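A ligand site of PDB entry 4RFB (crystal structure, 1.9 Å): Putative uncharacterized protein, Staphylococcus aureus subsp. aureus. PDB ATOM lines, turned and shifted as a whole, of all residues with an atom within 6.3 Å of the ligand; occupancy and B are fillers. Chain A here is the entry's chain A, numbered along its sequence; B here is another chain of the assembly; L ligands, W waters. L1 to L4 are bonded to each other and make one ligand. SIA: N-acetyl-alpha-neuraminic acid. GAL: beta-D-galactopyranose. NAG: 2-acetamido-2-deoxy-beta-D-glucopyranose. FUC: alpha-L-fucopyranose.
The backbone carbonyl oxygen of Asp 201 sits at hydrogen-bond distance from the backbone NH of Leu 148 (2.9 Å). NZ of Lys 192 lies within hydrogen-bond range of OE1 of Gln 195, at 2.7 Å. The guanidinium group (NH2) of Arg 198 sits at hydrogen-bond distance from the backbone carbonyl oxygen (O) of Thr 187 (2.8 Å).
Water W5 lies within hydrogen-bond range of O4 of SIA L1 (2.9 Å) and N of Phe 185 (3.3 Å).
Merely in contact with the ligand: Leu 148 (3.5 Å), Lys 184 (3.9 Å), Tyr 186 (3.5 Å), Glu 189 (3.6 Å) and Lys 73 of chain B (3.9996 Å). Hydrophobic or aromatic side chains that line the ligand: Leu 148, Phe 185, Tyr 186 and His 197. Of the 17 residues printed, 12 come within 4 Å of the ligand. Along chain A the residues within 4 Å of the ligand span positions 148 to 201. The nearest printed residue that does not touch the ligand is Gly 72 of chain B (5.2 Å).
An oxygen (O1B) of SIA L1 sits at hydrogen-bond distance from the side-chain hydroxyl (OG1) of Thr 187 (2.8 Å). An oxygen (O1A) of SIA L1 is in salt-bridge range of the guanidinium group (NH2) of Arg 198 (3.4 Å). The backbone NH (N) of Thr 187 sits at hydrogen-bond distance from an oxygen (O1A) of SIA L1. An oxygen (O2) of FUC L4 is in hydrogen-bond range of the side-chain amino group (NZ) of Lys 192 (2.7 Å). A ring nitrogen (NE2) of His 197 sits at hydrogen-bond distance from an oxygen (O6) of NAG L3, at 2.7 Å. The side-chain amide nitrogen of Gln 195 lies within hydrogen-bond range of an oxygen (O5) of NAG L3, at 3.0 Å. The side-chain carboxylate (OD2) of Asp 201 is in hydrogen-bond range of an oxygen (O9) of SIA L1 (2.7 Å). N5 of SIA L1 sits at hydrogen-bond distance from O of Phe 185 (2.9 Å).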
ATOM      1  N   LEU A 148      17.917   3.387 -28.457  1.00  0.00           N
ATOM      2  CA  LEU A 148      17.909   4.817 -28.677  1.00  0.00           C
ATOM      3  C   LEU A 148      18.329   5.121 -30.101  1.00  0.00           C
ATOM      4  O   LEU A 148      17.860   6.088 -30.695  1.00  0.00           O
ATOM      5  CB  LEU A 148      18.835   5.561 -27.679  1.00  0.00           C
ATOM      6  CG  LEU A 148      18.372   5.518 -26.206  1.00  0.00           C
ATOM      7  CD1 LEU A 148      19.276   6.385 -25.346  1.00  0.00           C
ATOM      8  CD2 LEU A 148      16.928   5.980 -26.041  1.00  0.00           C
ATOM      9  N   VAL A 177      12.365  14.994 -27.039  1.00  0.00           N
ATOM     10  CA  VAL A 177      12.350  14.418 -25.707  1.00  0.00           C
ATOM     11  C   VAL A 177      11.344  13.276 -25.662  1.00  0.00           C
ATOM     12  O   VAL A 177      10.166  13.481 -25.924  1.00  0.00           O
ATOM     13  CB  VAL A 177      11.979  15.445 -24.616  1.00  0.00           C
ATOM     14  CG1 VAL A 177      12.181  14.819 -23.254  1.00  0.00           C
ATOM     15  CG2 VAL A 177      12.855  16.680 -24.734  1.00  0.00           C
ATOM     16  N   LYS A 184      10.949   9.291 -16.029  1.00  0.00           N
ATOM     17  CA  LYS A 184      12.123   9.204 -16.902  1.00  0.00           C
ATOM     18  C   LYS A 184      11.945   9.801 -18.308  1.00  0.00           C
ATOM     19  O   LYS A 184      10.845   9.785 -18.880  1.00  0.00           O
ATOM     20  CB  LYS A 184      12.561   7.744 -16.989  1.00  0.00           C
ATOM     21  CG  LYS A 184      12.962   7.187 -15.620  1.00  0.00           C
ATOM     22  CD  LYS A 184      13.342   5.728 -15.703  1.00  0.00           C
ATOM     23  CE  LYS A 184      13.400   5.114 -14.303  1.00  0.00           C
ATOM     24  NZ  LYS A 184      14.457   5.732 -13.460  1.00  0.00           N
ATOM     25  N   PHE A 185      13.041  10.349 -18.844  1.00  0.00           N
ATOM     26  CA  PHE A 185      13.059  10.864 -20.195  1.00  0.00           C
ATOM     27  C   PHE A 185      14.423  10.680 -20.823  1.00  0.00           C
ATOM     28  O   PHE A 185      15.441  10.441 -20.125  1.00  0.00           O
ATOM     29  CB  PHE A 185      12.629  12.336 -20.270  1.00  0.00           C
ATOM     30  CG  PHE A 185      13.558  13.282 -19.544  1.00  0.00           C
ATOM     31  CD1 PHE A 185      14.609  13.885 -20.213  1.00  0.00           C
ATOM     32  CD2 PHE A 185      13.362  13.594 -18.214  1.00  0.00           C
ATOM     33  CE1 PHE A 185      15.484  14.761 -19.556  1.00  0.00           C
ATOM     34  CE2 PHE A 185      14.232  14.468 -17.522  1.00  0.00           C
ATOM     35  CZ  PHE A 185      15.303  15.041 -18.201  1.00  0.00           C
ATOM     36  N   TYR A 186      14.443  10.784 -22.159  1.00  0.00           N
ATOM     37  CA  TYR A 186      15.646  10.647 -22.948  1.00  0.00           C
ATOM     38  C   TYR A 186      15.621  11.768 -23.987  1.00  0.00           C
ATOM     39  O   TYR A 186      14.577  12.047 -24.588  1.00  0.00           O
ATOM     40  CB  TYR A 186      15.671   9.289 -23.627  1.00  0.00           C
ATOM     41  CG  TYR A 186      15.582   8.196 -22.615  1.00  0.00           C
ATOM     42  CD1 TYR A 186      16.709   7.688 -22.016  1.00  0.00           C
ATOM     43  CD2 TYR A 186      14.339   7.723 -22.214  1.00  0.00           C
ATOM     44  CE1 TYR A 186      16.622   6.690 -21.042  1.00  0.00           C
ATOM     45  CE2 TYR A 186      14.260   6.731 -21.250  1.00  0.00           C
ATOM     46  CZ  TYR A 186      15.376   6.230 -20.676  1.00  0.00           C
ATOM     47  OH  TYR A 186      15.236   5.272 -19.713  1.00  0.00           O
ATOM     48  N   THR A 187      16.737  12.436 -24.166  1.00  0.00           N
ATOM     49  CA  THR A 187      16.786  13.576 -25.088  1.00  0.00           C
ATOM     50  C   THR A 187      17.730  13.378 -26.267  1.00  0.00           C
ATOM     51  O   THR A 187      18.814  12.798 -26.097  1.00  0.00           O
ATOM     52  CB  THR A 187      17.223  14.855 -24.357  1.00  0.00           C
ATOM     53  OG1 THR A 187      16.383  15.066 -23.216  1.00  0.00           O
ATOM     54  CG2 THR A 187      17.142  16.095 -25.254  1.00  0.00           C
ATOM     55  N   PHE A 188      17.296  13.800 -27.459  1.00  0.00           N
ATOM     56  CA  PHE A 188      18.148  13.806 -28.655  1.00  0.00           C
ATOM     57  C   PHE A 188      18.263  15.286 -29.072  1.00  0.00           C
ATOM     58  O   PHE A 188      17.261  15.918 -29.346  1.00  0.00           O
ATOM     59  CB  PHE A 188      17.549  12.967 -29.803  1.00  0.00           C
ATOM     60  CG  PHE A 188      17.128  11.595 -29.397  1.00  0.00           C
ATOM     61  CD1 PHE A 188      18.005  10.749 -28.740  1.00  0.00           C
ATOM     62  CD2 PHE A 188      15.847  11.123 -29.713  1.00  0.00           C
ATOM     63  CE1 PHE A 188      17.618   9.460 -28.390  1.00  0.00           C
ATOM     64  CE2 PHE A 188      15.444   9.849 -29.360  1.00  0.00           C
ATOM     65  CZ  PHE A 188      16.322   9.022 -28.673  1.00  0.00           C
ATOM     66  N   GLU A 189      19.485  15.815 -29.083  1.00  0.00           N
ATOM     67  CA  GLU A 189      19.763  17.206 -29.457  1.00  0.00           C
ATOM     68  C   GLU A 189      19.926  17.289 -30.971  1.00  0.00           C
ATOM     69  O   GLU A 189      20.786  16.598 -31.537  1.00  0.00           O
ATOM     70  CB  GLU A 189      21.064  17.658 -28.776  1.00  0.00           C
ATOM     71  CG  GLU A 189      20.944  17.852 -27.281  1.00  0.00           C
ATOM     72  CD  GLU A 189      20.074  19.059 -26.897  1.00  0.00           C
ATOM     73  OE1 GLU A 189      19.917  19.993 -27.728  1.00  0.00           O
ATOM     74  OE2 GLU A 189      19.540  19.063 -25.766  1.00  0.00           O
ATOM     75  N   LYS A 192      23.500  17.892 -32.901  1.00  0.00           N
ATOM     76  CA  LYS A 192      24.575  16.909 -32.991  1.00  0.00           C
ATOM     77  C   LYS A 192      24.049  15.516 -33.277  1.00  0.00           C
ATOM     78  O   LYS A 192      22.886  15.246 -33.080  1.00  0.00           O
ATOM     79  CB  LYS A 192      25.423  16.894 -31.703  1.00  0.00           C
ATOM     80  CG  LYS A 192      24.659  16.659 -30.437  1.00  0.00           C
ATOM     81  CD  LYS A 192      25.553  16.606 -29.190  1.00  0.00           C
ATOM     82  CE  LYS A 192      24.685  16.201 -28.016  1.00  0.00           C
ATOM     83  NZ  LYS A 192      25.359  15.747 -26.767  1.00  0.00           N
ATOM     84  N   LEU A 194      23.563  11.629 -32.582  1.00  0.00           N
ATOM     85  CA  LEU A 194      23.474  10.824 -31.356  1.00  0.00           C
ATOM     86  C   LEU A 194      24.856  10.224 -31.097  1.00  0.00           C
ATOM     87  O   LEU A 194      25.504   9.711 -32.020  1.00  0.00           O
ATOM     88  CB  LEU A 194      22.469   9.711 -31.538  1.00  0.00           C
ATOM     89  CG  LEU A 194      22.267   8.803 -30.338  1.00  0.00           C
ATOM     90  CD1 LEU A 194      21.797   9.548 -29.090  1.00  0.00           C
ATOM     91  CD2 LEU A 194      21.288   7.710 -30.761  1.00  0.00           C
ATOM     92  N   GLN A 195      25.309  10.267 -29.858  1.00  0.00           N
ATOM     93  CA  GLN A 195      26.658   9.774 -29.599  1.00  0.00           C
ATOM     94  C   GLN A 195      26.723   8.257 -29.601  1.00  0.00           C
ATOM     95  O   GLN A 195      25.767   7.575 -29.178  1.00  0.00           O
ATOM     96  CB  GLN A 195      27.165  10.345 -28.311  1.00  0.00           C
ATOM     97  CG  GLN A 195      27.218  11.857 -28.374  1.00  0.00           C
ATOM     98  CD  GLN A 195      27.034  12.469 -27.008  1.00  0.00           C
ATOM     99  OE1 GLN A 195      26.055  13.156 -26.751  1.00  0.00           O
ATOM    100  NE2 GLN A 195      27.945  12.148 -26.106  1.00  0.00           N
ATOM    101  N   HIS A 197      28.152   5.996 -27.835  1.00  0.00           N
ATOM    102  CA  HIS A 197      27.949   5.239 -26.606  1.00  0.00           C
ATOM    103  C   HIS A 197      26.513   5.199 -26.148  1.00  0.00           C
ATOM    104  O   HIS A 197      26.235   4.517 -25.201  1.00  0.00           O
ATOM    105  CB  HIS A 197      28.821   5.760 -25.453  1.00  0.00           C
ATOM    106  CG  HIS A 197      28.486   7.153 -25.039  1.00  0.00           C
ATOM    107  ND1 HIS A 197      28.976   8.249 -25.696  1.00  0.00           N
ATOM    108  CD2 HIS A 197      27.671   7.624 -24.066  1.00  0.00           C
ATOM    109  CE1 HIS A 197      28.500   9.347 -25.125  1.00  0.00           C
ATOM    110  NE2 HIS A 197      27.699   8.985 -24.138  1.00  0.00           N
ATOM    111  N   ARG A 198      25.619   5.965 -26.780  1.00  0.00           N
ATOM    112  CA  ARG A 198      24.200   5.955 -26.459  1.00  0.00           C
ATOM    113  C   ARG A 198      23.407   5.107 -27.454  1.00  0.00           C
ATOM    114  O   ARG A 198      22.250   4.758 -27.194  1.00  0.00           O
ATOM    115  CB  ARG A 198      23.614   7.374 -26.412  1.00  0.00           C
ATOM    116  CG  ARG A 198      24.158   8.290 -25.346  1.00  0.00           C
ATOM    117  CD  ARG A 198      23.584   9.672 -25.445  1.00  0.00           C
ATOM    118  NE  ARG A 198      22.141   9.634 -25.145  1.00  0.00           N
ATOM    119  CZ  ARG A 198      21.254  10.525 -25.574  1.00  0.00           C
ATOM    120  NH1 ARG A 198      21.605  11.517 -26.383  1.00  0.00           N
ATOM    121  NH2 ARG A 198      19.996  10.388 -25.228  1.00  0.00           N
ATOM    122  N   ASP A 201      21.989   1.842 -26.042  1.00  0.00           N
ATOM    123  CA  ASP A 201      21.100   1.895 -24.883  1.00  0.00           C
ATOM    124  C   ASP A 201      19.692   1.529 -25.343  1.00  0.00           C
ATOM    125  O   ASP A 201      19.291   1.913 -26.432  1.00  0.00           O
ATOM    126  CB  ASP A 201      21.080   3.296 -24.266  1.00  0.00           C
ATOM    127  CG  ASP A 201      22.394   3.676 -23.621  1.00  0.00           C
ATOM    128  OD1 ASP A 201      23.278   2.813 -23.384  1.00  0.00           O
ATOM    129  OD2 ASP A 201      22.538   4.875 -23.326  1.00  0.00           O
ATOM    130  N   GLY B  72      34.347  11.628 -28.446  1.00  0.00           N
ATOM    131  CA  GLY B  72      33.845  12.880 -27.914  1.00  0.00           C
ATOM    132  C   GLY B  72      34.504  14.083 -28.578  1.00  0.00           C
ATOM    133  O   GLY B  72      34.606  14.141 -29.805  1.00  0.00           O
ATOM    134  N   LYS B  73      34.974  15.015 -27.755  1.00  0.00           N
ATOM    135  CA  LYS B  73      35.571  16.253 -28.275  1.00  0.00           C
ATOM    136  C   LYS B  73      37.050  16.113 -28.733  1.00  0.00           C
ATOM    137  O   LYS B  73      37.602  17.030 -29.334  1.00  0.00           O
ATOM    138  CB  LYS B  73      35.379  17.372 -27.248  1.00  0.00           C
ATOM    139  CG  LYS B  73      33.903  17.584 -26.916  1.00  0.00           C
ATOM    140  CD  LYS B  73      33.665  18.744 -25.953  1.00  0.00           C
ATOM    141  CE  LYS B  73      33.980  20.083 -26.585  1.00  0.00           C
ATOM    142  NZ  LYS B  73      33.826  21.182 -25.607  1.00  0.00           N
ATOM    143  N   GLU B  76      37.703  16.991 -32.286  1.00  0.00           N
ATOM    144  CA  GLU B  76      37.762  18.398 -32.649  1.00  0.00           C
ATOM    145  C   GLU B  76      39.167  19.000 -32.789  1.00  0.00           C
ATOM    146  O   GLU B  76      39.325  20.077 -33.377  1.00  0.00           O
ATOM    147  CB  GLU B  76      36.934  19.238 -31.683  1.00  0.00           C
ATOM    148  CG  GLU B  76      35.442  18.888 -31.687  1.00  0.00           C
ATOM    149  CD  GLU B  76      34.642  19.739 -30.722  1.00  0.00           C
ATOM    150  OE1 GLU B  76      35.227  20.694 -30.156  1.00  0.00           O
ATOM    151  OE2 GLU B  76      33.451  19.449 -30.517  1.00  0.00           O
HETATM  152  C1  SIA L   1      18.804  12.765 -21.512  1.00  0.00           C
HETATM  153  C2  SIA L   1      19.813  12.575 -20.400  1.00  0.00           C
HETATM  154  C3  SIA L   1      19.171  12.991 -19.048  1.00  0.00           C
HETATM  155  C4  SIA L   1      18.106  12.011 -18.580  1.00  0.00           C
HETATM  156  C5  SIA L   1      18.622  10.576 -18.631  1.00  0.00           C
HETATM  157  C6  SIA L   1      19.211  10.295 -20.016  1.00  0.00           C
HETATM  158  C7  SIA L   1      19.880   8.937 -20.188  1.00  0.00           C
HETATM  159  C8  SIA L   1      20.593   8.864 -21.553  1.00  0.00           C
HETATM  160  C9  SIA L   1      20.928   7.421 -21.934  1.00  0.00           C
HETATM  161  C10 SIA L   1      17.638   8.681 -17.414  1.00  0.00           C
HETATM  162  C11 SIA L   1      16.446   7.784 -17.323  1.00  0.00           C
HETATM  163  N5  SIA L   1      17.576   9.615 -18.353  1.00  0.00           N
HETATM  164  O1A SIA L   1      18.877  11.985 -22.480  1.00  0.00           O
HETATM  165  O1B SIA L   1      18.018  13.721 -21.452  1.00  0.00           O
HETATM  166  O4  SIA L   1      17.667  12.302 -17.238  1.00  0.00           O
HETATM  167  O6  SIA L   1      20.234  11.246 -20.327  1.00  0.00           O
HETATM  168  O7  SIA L   1      20.895   8.746 -19.168  1.00  0.00           O
HETATM  169  O8  SIA L   1      19.757   9.437 -22.529  1.00  0.00           O
HETATM  170  O9  SIA L   1      21.750   7.406 -23.107  1.00  0.00           O
HETATM  171  O10 SIA L   1      18.576   8.591 -16.635  1.00  0.00           O
HETATM  172  C1  GAL L   2      24.016  13.570 -22.459  1.00  0.00           C
HETATM  173  C2  GAL L   2      23.115  13.583 -21.234  1.00  0.00           C
HETATM  174  C3  GAL L   2      21.646  13.354 -21.633  1.00  0.00           C
HETATM  175  C4  GAL L   2      21.287  14.237 -22.804  1.00  0.00           C
HETATM  176  C5  GAL L   2      22.293  14.123 -23.930  1.00  0.00           C
HETATM  177  C6  GAL L   2      21.888  14.981 -25.120  1.00  0.00           C
HETATM  178  O2  GAL L   2      23.557  12.603 -20.300  1.00  0.00           O
HETATM  179  O3  GAL L   2      20.793  13.604 -20.522  1.00  0.00           O
HETATM  180  O4  GAL L   2      21.111  15.556 -22.341  1.00  0.00           O
HETATM  181  O5  GAL L   2      23.598  14.456 -23.481  1.00  0.00           O
HETATM  182  O6  GAL L   2      22.857  14.820 -26.154  1.00  0.00           O
HETATM  183  C1  NAG L   3      29.112  13.518 -23.371  1.00  0.00           C
HETATM  184  C2  NAG L   3      28.325  14.614 -24.053  1.00  0.00           C
HETATM  185  C3  NAG L   3      27.111  14.968 -23.211  1.00  0.00           C
HETATM  186  C4  NAG L   3      26.313  13.726 -22.889  1.00  0.00           C
HETATM  187  C5  NAG L   3      27.226  12.658 -22.258  1.00  0.00           C
HETATM  188  C6  NAG L   3      26.507  11.364 -21.892  1.00  0.00           C
HETATM  189  C7  NAG L   3      29.042  16.330 -25.659  1.00  0.00           C
HETATM  190  C8  NAG L   3      29.838  17.582 -25.928  1.00  0.00           C
HETATM  191  N2  NAG L   3      29.075  15.826 -24.417  1.00  0.00           N
HETATM  192  O1  NAG L   3      30.157  13.137 -24.215  1.00  0.00           O
HETATM  193  O3  NAG L   3      26.360  15.921 -23.928  1.00  0.00           O
HETATM  194  O4  NAG L   3      25.281  14.026 -21.971  1.00  0.00           O
HETATM  195  O5  NAG L   3      28.301  12.384 -23.141  1.00  0.00           O
HETATM  196  O6  NAG L   3      25.943  10.768 -23.073  1.00  0.00           O
HETATM  197  O7  NAG L   3      28.419  15.805 -26.590  1.00  0.00           O
HETATM  198  C1  FUC L   4      26.554  17.250 -23.440  1.00  0.00           C
HETATM  199  C2  FUC L   4      25.736  18.214 -24.300  1.00  0.00           C
HETATM  200  C3  FUC L   4      24.267  17.920 -24.112  1.00  0.00           C
HETATM  201  C4  FUC L   4      23.955  18.129 -22.644  1.00  0.00           C
HETATM  202  C5  FUC L   4      24.814  17.195 -21.794  1.00  0.00           C
HETATM  203  C6  FUC L   4      24.544  17.392 -20.309  1.00  0.00           C
HETATM  204  O2  FUC L   4      26.024  18.108 -25.686  1.00  0.00           O
HETATM  205  O3  FUC L   4      23.496  18.782 -24.911  1.00  0.00           O
HETATM  206  O4  FUC L   4      24.191  19.487 -22.313  1.00  0.00           O
HETATM  207  O5  FUC L   4      26.207  17.366 -22.056  1.00  0.00           O
HETATM  208  O   HOH W   1      24.414   8.475 -21.556  1.00  0.00           O
HETATM  209  O   HOH W   2      20.171   5.810 -18.573  1.00  0.00           O
HETATM  210  O   HOH W   3      17.271  12.614 -14.448  1.00  0.00           O
HETATM  211  O   HOH W   4      18.880  16.401 -20.886  1.00  0.00           O
HETATM  212  O   HOH W   5      15.152  11.104 -16.473  1.00  0.00           O
HETATM  213  O   HOH W   6      22.904  10.572 -18.987  1.00  0.00           O
HETATM  214  O   HOH W   7      26.619  21.086 -21.869  1.00  0.00           O
